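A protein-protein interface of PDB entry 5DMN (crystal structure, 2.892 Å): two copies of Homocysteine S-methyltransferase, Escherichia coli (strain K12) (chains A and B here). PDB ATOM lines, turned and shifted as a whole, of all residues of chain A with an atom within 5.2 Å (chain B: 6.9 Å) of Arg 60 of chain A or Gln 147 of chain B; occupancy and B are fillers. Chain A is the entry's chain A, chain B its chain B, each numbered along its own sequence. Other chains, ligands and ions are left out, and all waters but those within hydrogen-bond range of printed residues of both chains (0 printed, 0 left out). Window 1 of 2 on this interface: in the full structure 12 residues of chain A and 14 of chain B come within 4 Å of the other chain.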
ATOM      1  N   HIS A  55      -0.957   7.901   4.798  1.00  0.00           N
ATOM      2  CA  HIS A  55      -2.042   7.146   4.185  1.00  0.00           C
ATOM      3  C   HIS A  55      -1.544   5.798   3.685  1.00  0.00           C
ATOM      4  O   HIS A  55      -2.240   4.793   3.804  1.00  0.00           O
ATOM      5  CB  HIS A  55      -2.684   7.942   3.043  1.00  0.00           C
ATOM      6  CG  HIS A  55      -3.563   9.062   3.516  1.00  0.00           C
ATOM      7  ND1 HIS A  55      -3.607  10.289   2.888  1.00  0.00           N
ATOM      8  CD2 HIS A  55      -4.422   9.140   4.555  1.00  0.00           C
ATOM      9  CE1 HIS A  55      -4.463  11.072   3.522  1.00  0.00           C
ATOM     10  NE2 HIS A  55      -4.971  10.401   4.538  1.00  0.00           N
ATOM     11  N   LEU A  56      -0.332   5.779   3.146  1.00  0.00           N
ATOM     12  CA  LEU A  56       0.267   4.541   2.669  1.00  0.00           C
ATOM     13  C   LEU A  56       0.478   3.556   3.820  1.00  0.00           C
ATOM     14  O   LEU A  56       0.305   2.348   3.659  1.00  0.00           O
ATOM     15  CB  LEU A  56       1.590   4.835   1.957  1.00  0.00           C
ATOM     16  CG  LEU A  56       2.252   3.661   1.234  1.00  0.00           C
ATOM     17  CD1 LEU A  56       1.312   3.064   0.201  1.00  0.00           C
ATOM     18  CD2 LEU A  56       3.542   4.104   0.576  1.00  0.00           C
ATOM     19  N   ASP A  57       0.835   4.085   4.986  1.00  0.00           N
ATOM     20  CA  ASP A  57       1.055   3.257   6.166  1.00  0.00           C
ATOM     21  C   ASP A  57      -0.225   2.551   6.602  1.00  0.00           C
ATOM     22  O   ASP A  57      -0.201   1.374   6.974  1.00  0.00           O
ATOM     23  CB  ASP A  57       1.597   4.100   7.322  1.00  0.00           C
ATOM     24  CG  ASP A  57       3.075   4.406   7.179  1.00  0.00           C
ATOM     25  OD1 ASP A  57       3.777   3.639   6.481  1.00  0.00           O
ATOM     26  OD2 ASP A  57       3.539   5.406   7.772  1.00  0.00           O
ATOM     27  N   TYR A  58      -1.341   3.276   6.556  1.00  0.00           N
ATOM     28  CA  TYR A  58      -2.611   2.719   7.000  1.00  0.00           C
ATOM     29  C   TYR A  58      -3.096   1.655   6.037  1.00  0.00           C
ATOM     30  O   TYR A  58      -3.637   0.634   6.456  1.00  0.00           O
ATOM     31  CB  TYR A  58      -3.662   3.811   7.157  1.00  0.00           C
ATOM     32  CG  TYR A  58      -3.661   4.449   8.527  1.00  0.00           C
ATOM     33  CD1 TYR A  58      -4.106   3.749   9.640  1.00  0.00           C
ATOM     34  CD2 TYR A  58      -3.223   5.757   8.708  1.00  0.00           C
ATOM     35  CE1 TYR A  58      -4.106   4.330  10.894  1.00  0.00           C
ATOM     36  CE2 TYR A  58      -3.224   6.348   9.956  1.00  0.00           C
ATOM     37  CZ  TYR A  58      -3.670   5.631  11.045  1.00  0.00           C
ATOM     38  OH  TYR A  58      -3.676   6.210  12.293  1.00  0.00           O
ATOM     39  N   TYR A  59      -2.900   1.890   4.747  1.00  0.00           N
ATOM     40  CA  TYR A  59      -3.224   0.880   3.751  1.00  0.00           C
ATOM     41  C   TYR A  59      -2.413  -0.381   4.004  1.00  0.00           C
ATOM     42  O   TYR A  59      -2.917  -1.492   3.850  1.00  0.00           O
ATOM     43  CB  TYR A  59      -2.966   1.415   2.348  1.00  0.00           C
ATOM     44  CG  TYR A  59      -4.087   2.284   1.833  1.00  0.00           C
ATOM     45  CD1 TYR A  59      -5.409   1.867   1.925  1.00  0.00           C
ATOM     46  CD2 TYR A  59      -3.830   3.535   1.289  1.00  0.00           C
ATOM     47  CE1 TYR A  59      -6.439   2.656   1.462  1.00  0.00           C
ATOM     48  CE2 TYR A  59      -4.854   4.333   0.828  1.00  0.00           C
ATOM     49  CZ  TYR A  59      -6.158   3.891   0.916  1.00  0.00           C
ATOM     50  OH  TYR A  59      -7.188   4.685   0.459  1.00  0.00           O
ATOM     51  N   ARG A  60      -1.162  -0.200   4.421  1.00  0.00           N
ATOM     52  CA  ARG A  60      -0.276  -1.322   4.717  1.00  0.00           C
ATOM     53  C   ARG A  60      -0.706  -2.079   5.975  1.00  0.00           C
ATOM     54  O   ARG A  60      -0.708  -3.311   6.000  1.00  0.00           O
ATOM     55  CB  ARG A  60       1.160  -0.826   4.876  1.00  0.00           C
ATOM     56  CG  ARG A  60       1.883  -0.598   3.568  1.00  0.00           C
ATOM     57  CD  ARG A  60       3.206   0.099   3.808  1.00  0.00           C
ATOM     58  NE  ARG A  60       3.935   0.357   2.570  1.00  0.00           N
ATOM     59  CZ  ARG A  60       4.877   1.284   2.446  1.00  0.00           C
ATOM     60  NH1 ARG A  60       5.190   2.053   3.482  1.00  0.00           N
ATOM     61  NH2 ARG A  60       5.494   1.455   1.286  1.00  0.00           N
ATOM     62  N   ALA A  61      -1.085  -1.331   7.009  1.00  0.00           N
ATOM     63  CA  ALA A  61      -1.521  -1.911   8.280  1.00  0.00           C
ATOM     64  C   ALA A  61      -2.812  -2.727   8.130  1.00  0.00           C
ATOM     65  O   ALA A  61      -3.148  -3.541   8.992  1.00  0.00           O
ATOM     66  CB  ALA A  61      -1.701  -0.818   9.318  1.00  0.00           C
ATOM     67  N   GLY A  62      -3.558  -2.469   7.062  1.00  0.00           N
ATOM     68  CA  GLY A  62      -4.730  -3.265   6.761  1.00  0.00           C
ATOM     69  C   GLY A  62      -6.000  -2.479   6.507  1.00  0.00           C
ATOM     70  O   GLY A  62      -7.055  -3.074   6.276  1.00  0.00           O
ATOM     71  N   TYR A 106      -0.017   1.718  -3.171  1.00  0.00           N
ATOM     72  CA  TYR A 106      -0.242   0.457  -2.481  1.00  0.00           C
ATOM     73  C   TYR A 106      -0.705  -0.626  -3.449  1.00  0.00           C
ATOM     74  O   TYR A 106      -0.368  -1.796  -3.286  1.00  0.00           O
ATOM     75  CB  TYR A 106      -1.257   0.629  -1.349  1.00  0.00           C
ATOM     76  CG  TYR A 106      -1.459  -0.629  -0.539  1.00  0.00           C
ATOM     77  CD1 TYR A 106      -0.493  -1.061   0.363  1.00  0.00           C
ATOM     78  CD2 TYR A 106      -2.609  -1.390  -0.678  1.00  0.00           C
ATOM     79  CE1 TYR A 106      -0.671  -2.216   1.103  1.00  0.00           C
ATOM     80  CE2 TYR A 106      -2.797  -2.544   0.058  1.00  0.00           C
ATOM     81  CZ  TYR A 106      -1.827  -2.955   0.944  1.00  0.00           C
ATOM     82  OH  TYR A 106      -2.017  -4.107   1.673  1.00  0.00           O
ATOM     83  N   GLU A 109       2.293  -2.078  -5.077  1.00  0.00           N
ATOM     84  CA  GLU A 109       3.029  -2.951  -4.167  1.00  0.00           C
ATOM     85  C   GLU A 109       2.333  -4.303  -4.008  1.00  0.00           C
ATOM     86  O   GLU A 109       2.924  -5.350  -4.277  1.00  0.00           O
ATOM     87  CB  GLU A 109       3.193  -2.274  -2.801  1.00  0.00           C
ATOM     88  CG  GLU A 109       3.893  -3.128  -1.752  1.00  0.00           C
ATOM     89  CD  GLU A 109       4.108  -2.386  -0.442  1.00  0.00           C
ATOM     90  OE1 GLU A 109       4.095  -1.132  -0.456  1.00  0.00           O
ATOM     91  OE2 GLU A 109       4.284  -3.059   0.601  1.00  0.00           O
ATOM     92  N   SER B 142       8.397  -7.510   0.842  1.00  0.00           N
ATOM     93  CA  SER B 142       7.653  -6.260   0.744  1.00  0.00           C
ATOM     94  C   SER B 142       7.777  -5.504   2.058  1.00  0.00           C
ATOM     95  O   SER B 142       8.009  -6.114   3.100  1.00  0.00           O
ATOM     96  CB  SER B 142       6.183  -6.518   0.413  1.00  0.00           C
ATOM     97  OG  SER B 142       5.509  -7.133   1.496  1.00  0.00           O
ATOM     98  N   VAL B 143       7.627  -4.182   2.007  1.00  0.00           N
ATOM     99  CA  VAL B 143       7.660  -3.359   3.213  1.00  0.00           C
ATOM    100  C   VAL B 143       6.688  -3.887   4.267  1.00  0.00           C
ATOM    101  O   VAL B 143       7.031  -3.994   5.447  1.00  0.00           O
ATOM    102  CB  VAL B 143       7.336  -1.885   2.899  1.00  0.00           C
ATOM    103  CG1 VAL B 143       7.089  -1.102   4.177  1.00  0.00           C
ATOM    104  CG2 VAL B 143       8.471  -1.263   2.107  1.00  0.00           C
ATOM    105  N   GLU B 144       5.486  -4.247   3.829  1.00  0.00           N
ATOM    106  CA  GLU B 144       4.470  -4.761   4.736  1.00  0.00           C
ATOM    107  C   GLU B 144       4.890  -6.101   5.332  1.00  0.00           C
ATOM    108  O   GLU B 144       4.530  -6.425   6.464  1.00  0.00           O
ATOM    109  CB  GLU B 144       3.133  -4.910   4.012  1.00  0.00           C
ATOM    110  CG  GLU B 144       2.016  -5.400   4.904  1.00  0.00           C
ATOM    111  CD  GLU B 144       0.893  -6.036   4.121  1.00  0.00           C
ATOM    112  OE1 GLU B 144       0.294  -7.012   4.627  1.00  0.00           O
ATOM    113  OE2 GLU B 144       0.612  -5.557   2.999  1.00  0.00           O
ATOM    114  N   ALA B 145       5.640  -6.884   4.563  1.00  0.00           N
ATOM    115  CA  ALA B 145       6.163  -8.155   5.054  1.00  0.00           C
ATOM    116  C   ALA B 145       7.207  -7.922   6.155  1.00  0.00           C
ATOM    117  O   ALA B 145       7.208  -8.602   7.180  1.00  0.00           O
ATOM    118  CB  ALA B 145       6.754  -8.963   3.915  1.00  0.00           C
ATOM    119  N   PHE B 146       8.095  -6.957   5.938  1.00  0.00           N
ATOM    120  CA  PHE B 146       9.058  -6.569   6.960  1.00  0.00           C
ATOM    121  C   PHE B 146       8.355  -6.034   8.211  1.00  0.00           C
ATOM    122  O   PHE B 146       8.749  -6.343   9.336  1.00  0.00           O
ATOM    123  CB  PHE B 146      10.028  -5.515   6.413  1.00  0.00           C
ATOM    124  CG  PHE B 146      11.003  -6.045   5.393  1.00  0.00           C
ATOM    125  CD1 PHE B 146      11.696  -7.224   5.620  1.00  0.00           C
ATOM    126  CD2 PHE B 146      11.227  -5.359   4.209  1.00  0.00           C
ATOM    127  CE1 PHE B 146      12.596  -7.708   4.684  1.00  0.00           C
ATOM    128  CE2 PHE B 146      12.121  -5.837   3.269  1.00  0.00           C
ATOM    129  CZ  PHE B 146      12.806  -7.012   3.506  1.00  0.00           C
ATOM    130  N   GLN B 147       7.308  -5.240   8.008  1.00  0.00           N
ATOM    131  CA  GLN B 147       6.596  -4.614   9.119  1.00  0.00           C
ATOM    132  C   GLN B 147       5.771  -5.639   9.901  1.00  0.00           C
ATOM    133  O   GLN B 147       5.676  -5.575  11.128  1.00  0.00           O
ATOM    134  CB  GLN B 147       5.711  -3.483   8.603  1.00  0.00           C
ATOM    135  CG  GLN B 147       6.498  -2.255   8.168  1.00  0.00           C
ATOM    136  CD  GLN B 147       5.612  -1.157   7.598  1.00  0.00           C
ATOM    137  OE1 GLN B 147       4.457  -1.393   7.246  1.00  0.00           O
ATOM    138  NE2 GLN B 147       6.157   0.050   7.497  1.00  0.00           N
ATOM    139  N   ALA B 148       5.180  -6.591   9.188  1.00  0.00           N
ATOM    140  CA  ALA B 148       4.429  -7.661   9.829  1.00  0.00           C
ATOM    141  C   ALA B 148       5.366  -8.562  10.629  1.00  0.00           C
ATOM    142  O   ALA B 148       5.004  -9.099  11.677  1.00  0.00           O
ATOM    143  CB  ALA B 148       3.674  -8.471   8.790  1.00  0.00           C
ATOM    144  N   PHE B 149       6.585  -8.712  10.129  1.00  0.00           N
ATOM    145  CA  PHE B 149       7.569  -9.562  10.777  1.00  0.00           C
ATOM    146  C   PHE B 149       8.054  -8.926  12.074  1.00  0.00           C
ATOM    147  O   PHE B 149       8.189  -9.601  13.091  1.00  0.00           O
ATOM    148  CB  PHE B 149       8.746  -9.820   9.831  1.00  0.00           C
ATOM    149  CG  PHE B 149       9.855 -10.627  10.442  1.00  0.00           C
ATOM    150  CD1 PHE B 149       9.829 -12.009  10.390  1.00  0.00           C
ATOM    151  CD2 PHE B 149      10.930 -10.005  11.059  1.00  0.00           C
ATOM    152  CE1 PHE B 149      10.848 -12.756  10.945  1.00  0.00           C
ATOM    153  CE2 PHE B 149      11.951 -10.749  11.619  1.00  0.00           C
ATOM    154  CZ  PHE B 149      11.910 -12.126  11.560  1.00  0.00           C
ATOM    155  N   HIS B 150       8.292  -7.617  12.037  1.00  0.00           N
ATOM    156  CA  HIS B 150       8.935  -6.925  13.147  1.00  0.00           C
ATOM    157  C   HIS B 150       7.953  -6.388  14.188  1.00  0.00           C
ATOM    158  O   HIS B 150       8.340  -6.116  15.326  1.00  0.00           O
ATOM    159  CB  HIS B 150       9.794  -5.772  12.618  1.00  0.00           C
ATOM    160  CG  HIS B 150      11.026  -6.218  11.888  1.00  0.00           C
ATOM    161  ND1 HIS B 150      11.951  -7.075  12.442  1.00  0.00           N
ATOM    162  CD2 HIS B 150      11.491  -5.909  10.654  1.00  0.00           C
ATOM    163  CE1 HIS B 150      12.929  -7.284  11.577  1.00  0.00           C
ATOM    164  NE2 HIS B 150      12.675  -6.588  10.485  1.00  0.00           N
ATOM    165  N   ARG B 151       6.689  -6.234  13.804  1.00  0.00           N
ATOM    166  CA  ARG B 151       5.698  -5.635  14.699  1.00  0.00           C
ATOM    167  C   ARG B 151       5.525  -6.373  16.043  1.00  0.00           C
ATOM    168  O   ARG B 151       5.457  -5.718  17.087  1.00  0.00           O
ATOM    169  CB  ARG B 151       4.345  -5.520  13.991  1.00  0.00           C
ATOM    170  CG  ARG B 151       3.441  -4.434  14.566  1.00  0.00           C
ATOM    171  CD  ARG B 151       2.047  -4.459  13.949  1.00  0.00           C
ATOM    172  NE  ARG B 151       2.096  -4.428  12.488  1.00  0.00           N
ATOM    173  CZ  ARG B 151       2.148  -3.316  11.763  1.00  0.00           C
ATOM    174  NH1 ARG B 151       2.189  -2.133  12.363  1.00  0.00           N
ATOM    175  NH2 ARG B 151       2.183  -3.386  10.439  1.00  0.00           N
ATOM    176  N   PRO B 152       5.454  -7.724  16.033  1.00  0.00           N
ATOM    177  CA  PRO B 152       5.389  -8.433  17.321  1.00  0.00           C
ATOM    178  C   PRO B 152       6.510  -8.063  18.295  1.00  0.00           C
ATOM    179  O   PRO B 152       6.256  -7.786  19.467  1.00  0.00           O
ATOM    180  CB  PRO B 152       5.514  -9.902  16.916  1.00  0.00           C
ATOM    181  CG  PRO B 152       4.938  -9.957  15.559  1.00  0.00           C
ATOM    182  CD  PRO B 152       5.301  -8.658  14.899  1.00  0.00           C
ATOM    183  N   GLU B 177      13.885   0.943   5.690  1.00  0.00           N
ATOM    184  CA  GLU B 177      12.752   1.861   5.504  1.00  0.00           C
ATOM    185  C   GLU B 177      11.544   1.411   6.298  1.00  0.00           C
ATOM    186  O   GLU B 177      10.947   2.194   7.039  1.00  0.00           O
ATOM    187  CB  GLU B 177      12.333   1.971   4.035  1.00  0.00           C
ATOM    188  CG  GLU B 177      13.452   2.161   3.039  1.00  0.00           C
ATOM    189  CD  GLU B 177      12.944   2.177   1.608  1.00  0.00           C
ATOM    190  OE1 GLU B 177      11.756   2.509   1.397  1.00  0.00           O
ATOM    191  OE2 GLU B 177      13.732   1.848   0.695  1.00  0.00           O
ATOM    192  N   ALA B 178      11.207   0.135   6.141  1.00  0.00           N
ATOM    193  CA  ALA B 178      10.020  -0.442   6.755  1.00  0.00           C
ATOM    194  C   ALA B 178      10.043  -0.284   8.260  1.00  0.00           C
ATOM    195  O   ALA B 178       9.000  -0.095   8.888  1.00  0.00           O
ATOM    196  CB  ALA B 178       9.897  -1.909   6.386  1.00  0.00           C
ATOM    197  N   LEU B 179      11.243  -0.354   8.824  1.00  0.00           N
ATOM    198  CA  LEU B 179      11.423  -0.270  10.262  1.00  0.00           C
ATOM    199  C   LEU B 179      11.261   1.161  10.763  1.00  0.00           C
ATOM    200  O   LEU B 179      10.640   1.403  11.799  1.00  0.00           O
ATOM    201  CB  LEU B 179      12.795  -0.813  10.639  1.00  0.00           C
ATOM    202  CG  LEU B 179      12.812  -1.725  11.858  1.00  0.00           C
ATOM    203  CD1 LEU B 179      11.641  -2.697  11.782  1.00  0.00           C
ATOM    204  CD2 LEU B 179      14.140  -2.475  11.935  1.00  0.00           C
ATOM    205  N   ALA B 180      11.804   2.113  10.011  1.00  0.00           N
ATOM    206  CA  ALA B 180      11.684   3.513  10.380  1.00  0.00           C
ATOM    207  C   ALA B 180      10.224   3.942  10.273  1.00  0.00           C
ATOM    208  O   ALA B 180       9.748   4.759  11.066  1.00  0.00           O
ATOM    209  CB  ALA B 180      12.571   4.378   9.502  1.00  0.00           C
ATOM    210  N   GLU B 181       9.516   3.385   9.291  1.00  0.00           N
ATOM    211  CA  GLU B 181       8.096   3.674   9.129  1.00  0.00           C
ATOM    212  C   GLU B 181       7.293   3.035  10.247  1.00  0.00           C
ATOM    213  O   GLU B 181       6.479   3.695  10.888  1.00  0.00           O
ATOM    214  CB  GLU B 181       7.585   3.185   7.771  1.00  0.00           C
ATOM    215  CG  GLU B 181       7.813   4.164   6.623  1.00  0.00           C
ATOM    216  CD  GLU B 181       7.051   5.472   6.796  1.00  0.00           C
ATOM    217  OE1 GLU B 181       5.804   5.463   6.716  1.00  0.00           O
ATOM    218  OE2 GLU B 181       7.703   6.518   7.011  1.00  0.00           O
ATOM    219  N   LEU B 182       7.553   1.756  10.497  1.00  0.00           N
ATOM    220  CA  LEU B 182       6.891   1.025  11.572  1.00  0.00           C
ATOM    221  C   LEU B 182       6.983   1.766  12.897  1.00  0.00           C
ATOM    222  O   LEU B 182       6.027   1.781  13.666  1.00  0.00           O
ATOM    223  CB  LEU B 182       7.501  -0.370  11.720  1.00  0.00           C
ATOM    224  CG  LEU B 182       7.044  -1.230  12.899  1.00  0.00           C
ATOM    225  CD1 LEU B 182       5.565  -1.553  12.816  1.00  0.00           C
ATOM    226  CD2 LEU B 182       7.874  -2.503  12.997  1.00  0.00           C
ATOM    227  N   LEU B 183       8.124   2.405  13.147  1.00  0.00           N
ATOM    228  CA  LEU B 183       8.346   3.098  14.412  1.00  0.00           C
ATOM    229  C   LEU B 183       7.394   4.271  14.608  1.00  0.00           C
ATOM    230  O   LEU B 183       7.032   4.599  15.738  1.00  0.00           O
ATOM    231  CB  LEU B 183       9.788   3.597  14.507  1.00  0.00           C
ATOM    232  CG  LEU B 183      10.895   2.599  14.838  1.00  0.00           C
ATOM    233  CD1 LEU B 183      12.243   3.303  14.777  1.00  0.00           C
ATOM    234  CD2 LEU B 183      10.686   1.956  16.203  1.00  0.00           C
ATOM    235  N   TYR B 186       4.442   4.187  16.808  1.00  0.00           N
ATOM    236  CA  TYR B 186       4.610   4.297  18.253  1.00  0.00           C
ATOM    237  C   TYR B 186       5.375   5.576  18.575  1.00  0.00           C
ATOM    238  O   TYR B 186       6.593   5.554  18.740  1.00  0.00           O
ATOM    239  CB  TYR B 186       5.328   3.062  18.794  1.00  0.00           C
ATOM    240  CG  TYR B 186       4.836   1.806  18.123  1.00  0.00           C
ATOM    241  CD1 TYR B 186       5.502   1.280  17.024  1.00  0.00           C
ATOM    242  CD2 TYR B 186       3.690   1.166  18.561  1.00  0.00           C
ATOM    243  CE1 TYR B 186       5.042   0.147  16.389  1.00  0.00           C
ATOM    244  CE2 TYR B 186       3.222   0.029  17.930  1.00  0.00           C
ATOM    245  CZ  TYR B 186       3.903  -0.476  16.847  1.00  0.00           C
ATOM    246  OH  TYR B 186       3.447  -1.610  16.219  1.00  0.00           O
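The side-chain hydroxyl of Tyr 106 of chain A lies within hydrogen-bond range of the side-chain carboxylate of Glu 144 of chain B (3.3 Å).
OE1 of Glu 181 of chain B lies close to OD2 of Asp 57 of chain A, 2.5 Å away.
The guanidinium group (NH1) of Arg 60 of chain A lies within salt-bridge range of the side-chain carboxylate (OD1) of Asp 57 of chain A (3.7 Å).
NE of Arg 60 of chain A lies within salt-bridge range of OE1 of Glu 109 of chain A.
The side-chain amide nitrogen of Gln 147 of chain B is in hydrogen-bond range of the backbone carbonyl oxygen of Ala 178 of chain B (3.2 Å).
N of Ala 145 of chain B lies within hydrogen-bond range of OG of Ser 142 of chain B.
Among the printed residues, merely in contact across the chains: Arg 60 of chain A with Glu 144 of chain B, Glu 109 of chain A with Glu 144 of chain B, Arg 60 of chain A with Val 143 of chain B, Glu 109 of chain A with Val 143 of chain B, Glu 109 of chain A with Ser 142 of chain B and Arg 60 of chain A with Gln 147 of chain B.
Of the printed residues of chain B, Arg 60 of chain A touches Val 143 (3.7 Å), Glu 144 (3.6 Å) and Gln 147 (3.95 Å).
Of chain A, only Arg 60 (3.95 Å) comes within 4 Å of Gln 147 of chain B.
Of the printed residues of chain B, Tyr 106 of chain A touches Glu 144.
Printed residues of chain A within 4 Å of Val 143 of chain B: Arg 60 and Glu 109.
The nearest residue of chain B that does not touch Arg 60 of chain A is Glu 181 of chain B (4.6 Å).
The nearest residue of chain A that does not touch Gln 147 of chain B is Asp 57 of chain A (4.4 Å).
The nearest printed residue of chain B that does not touch Glu 109 of chain A is Ala 145 of chain B (5.7 Å).
Of the 19 printed residues of chain B, 5 touch a printed residue of chain A.
Printed residues of chain B that touch a printed residue of chain A: Ser 142, Val 143, Glu 144, Gln 147 and Glu 181.
Of the 10 printed residues of chain A, 4 touch a printed residue of chain B.
Among the printed residues, 8 pairs touch across the chains.
Among the printed residues, no Asp or Glu carboxylate lies within 4 Å of a Lys or Arg side-chain nitrogen of the other chain.
No position is printed for both chains.
Of the 8 pairs that touch across the chains among the printed residues, none has its exchanged pair printed and touching as well.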
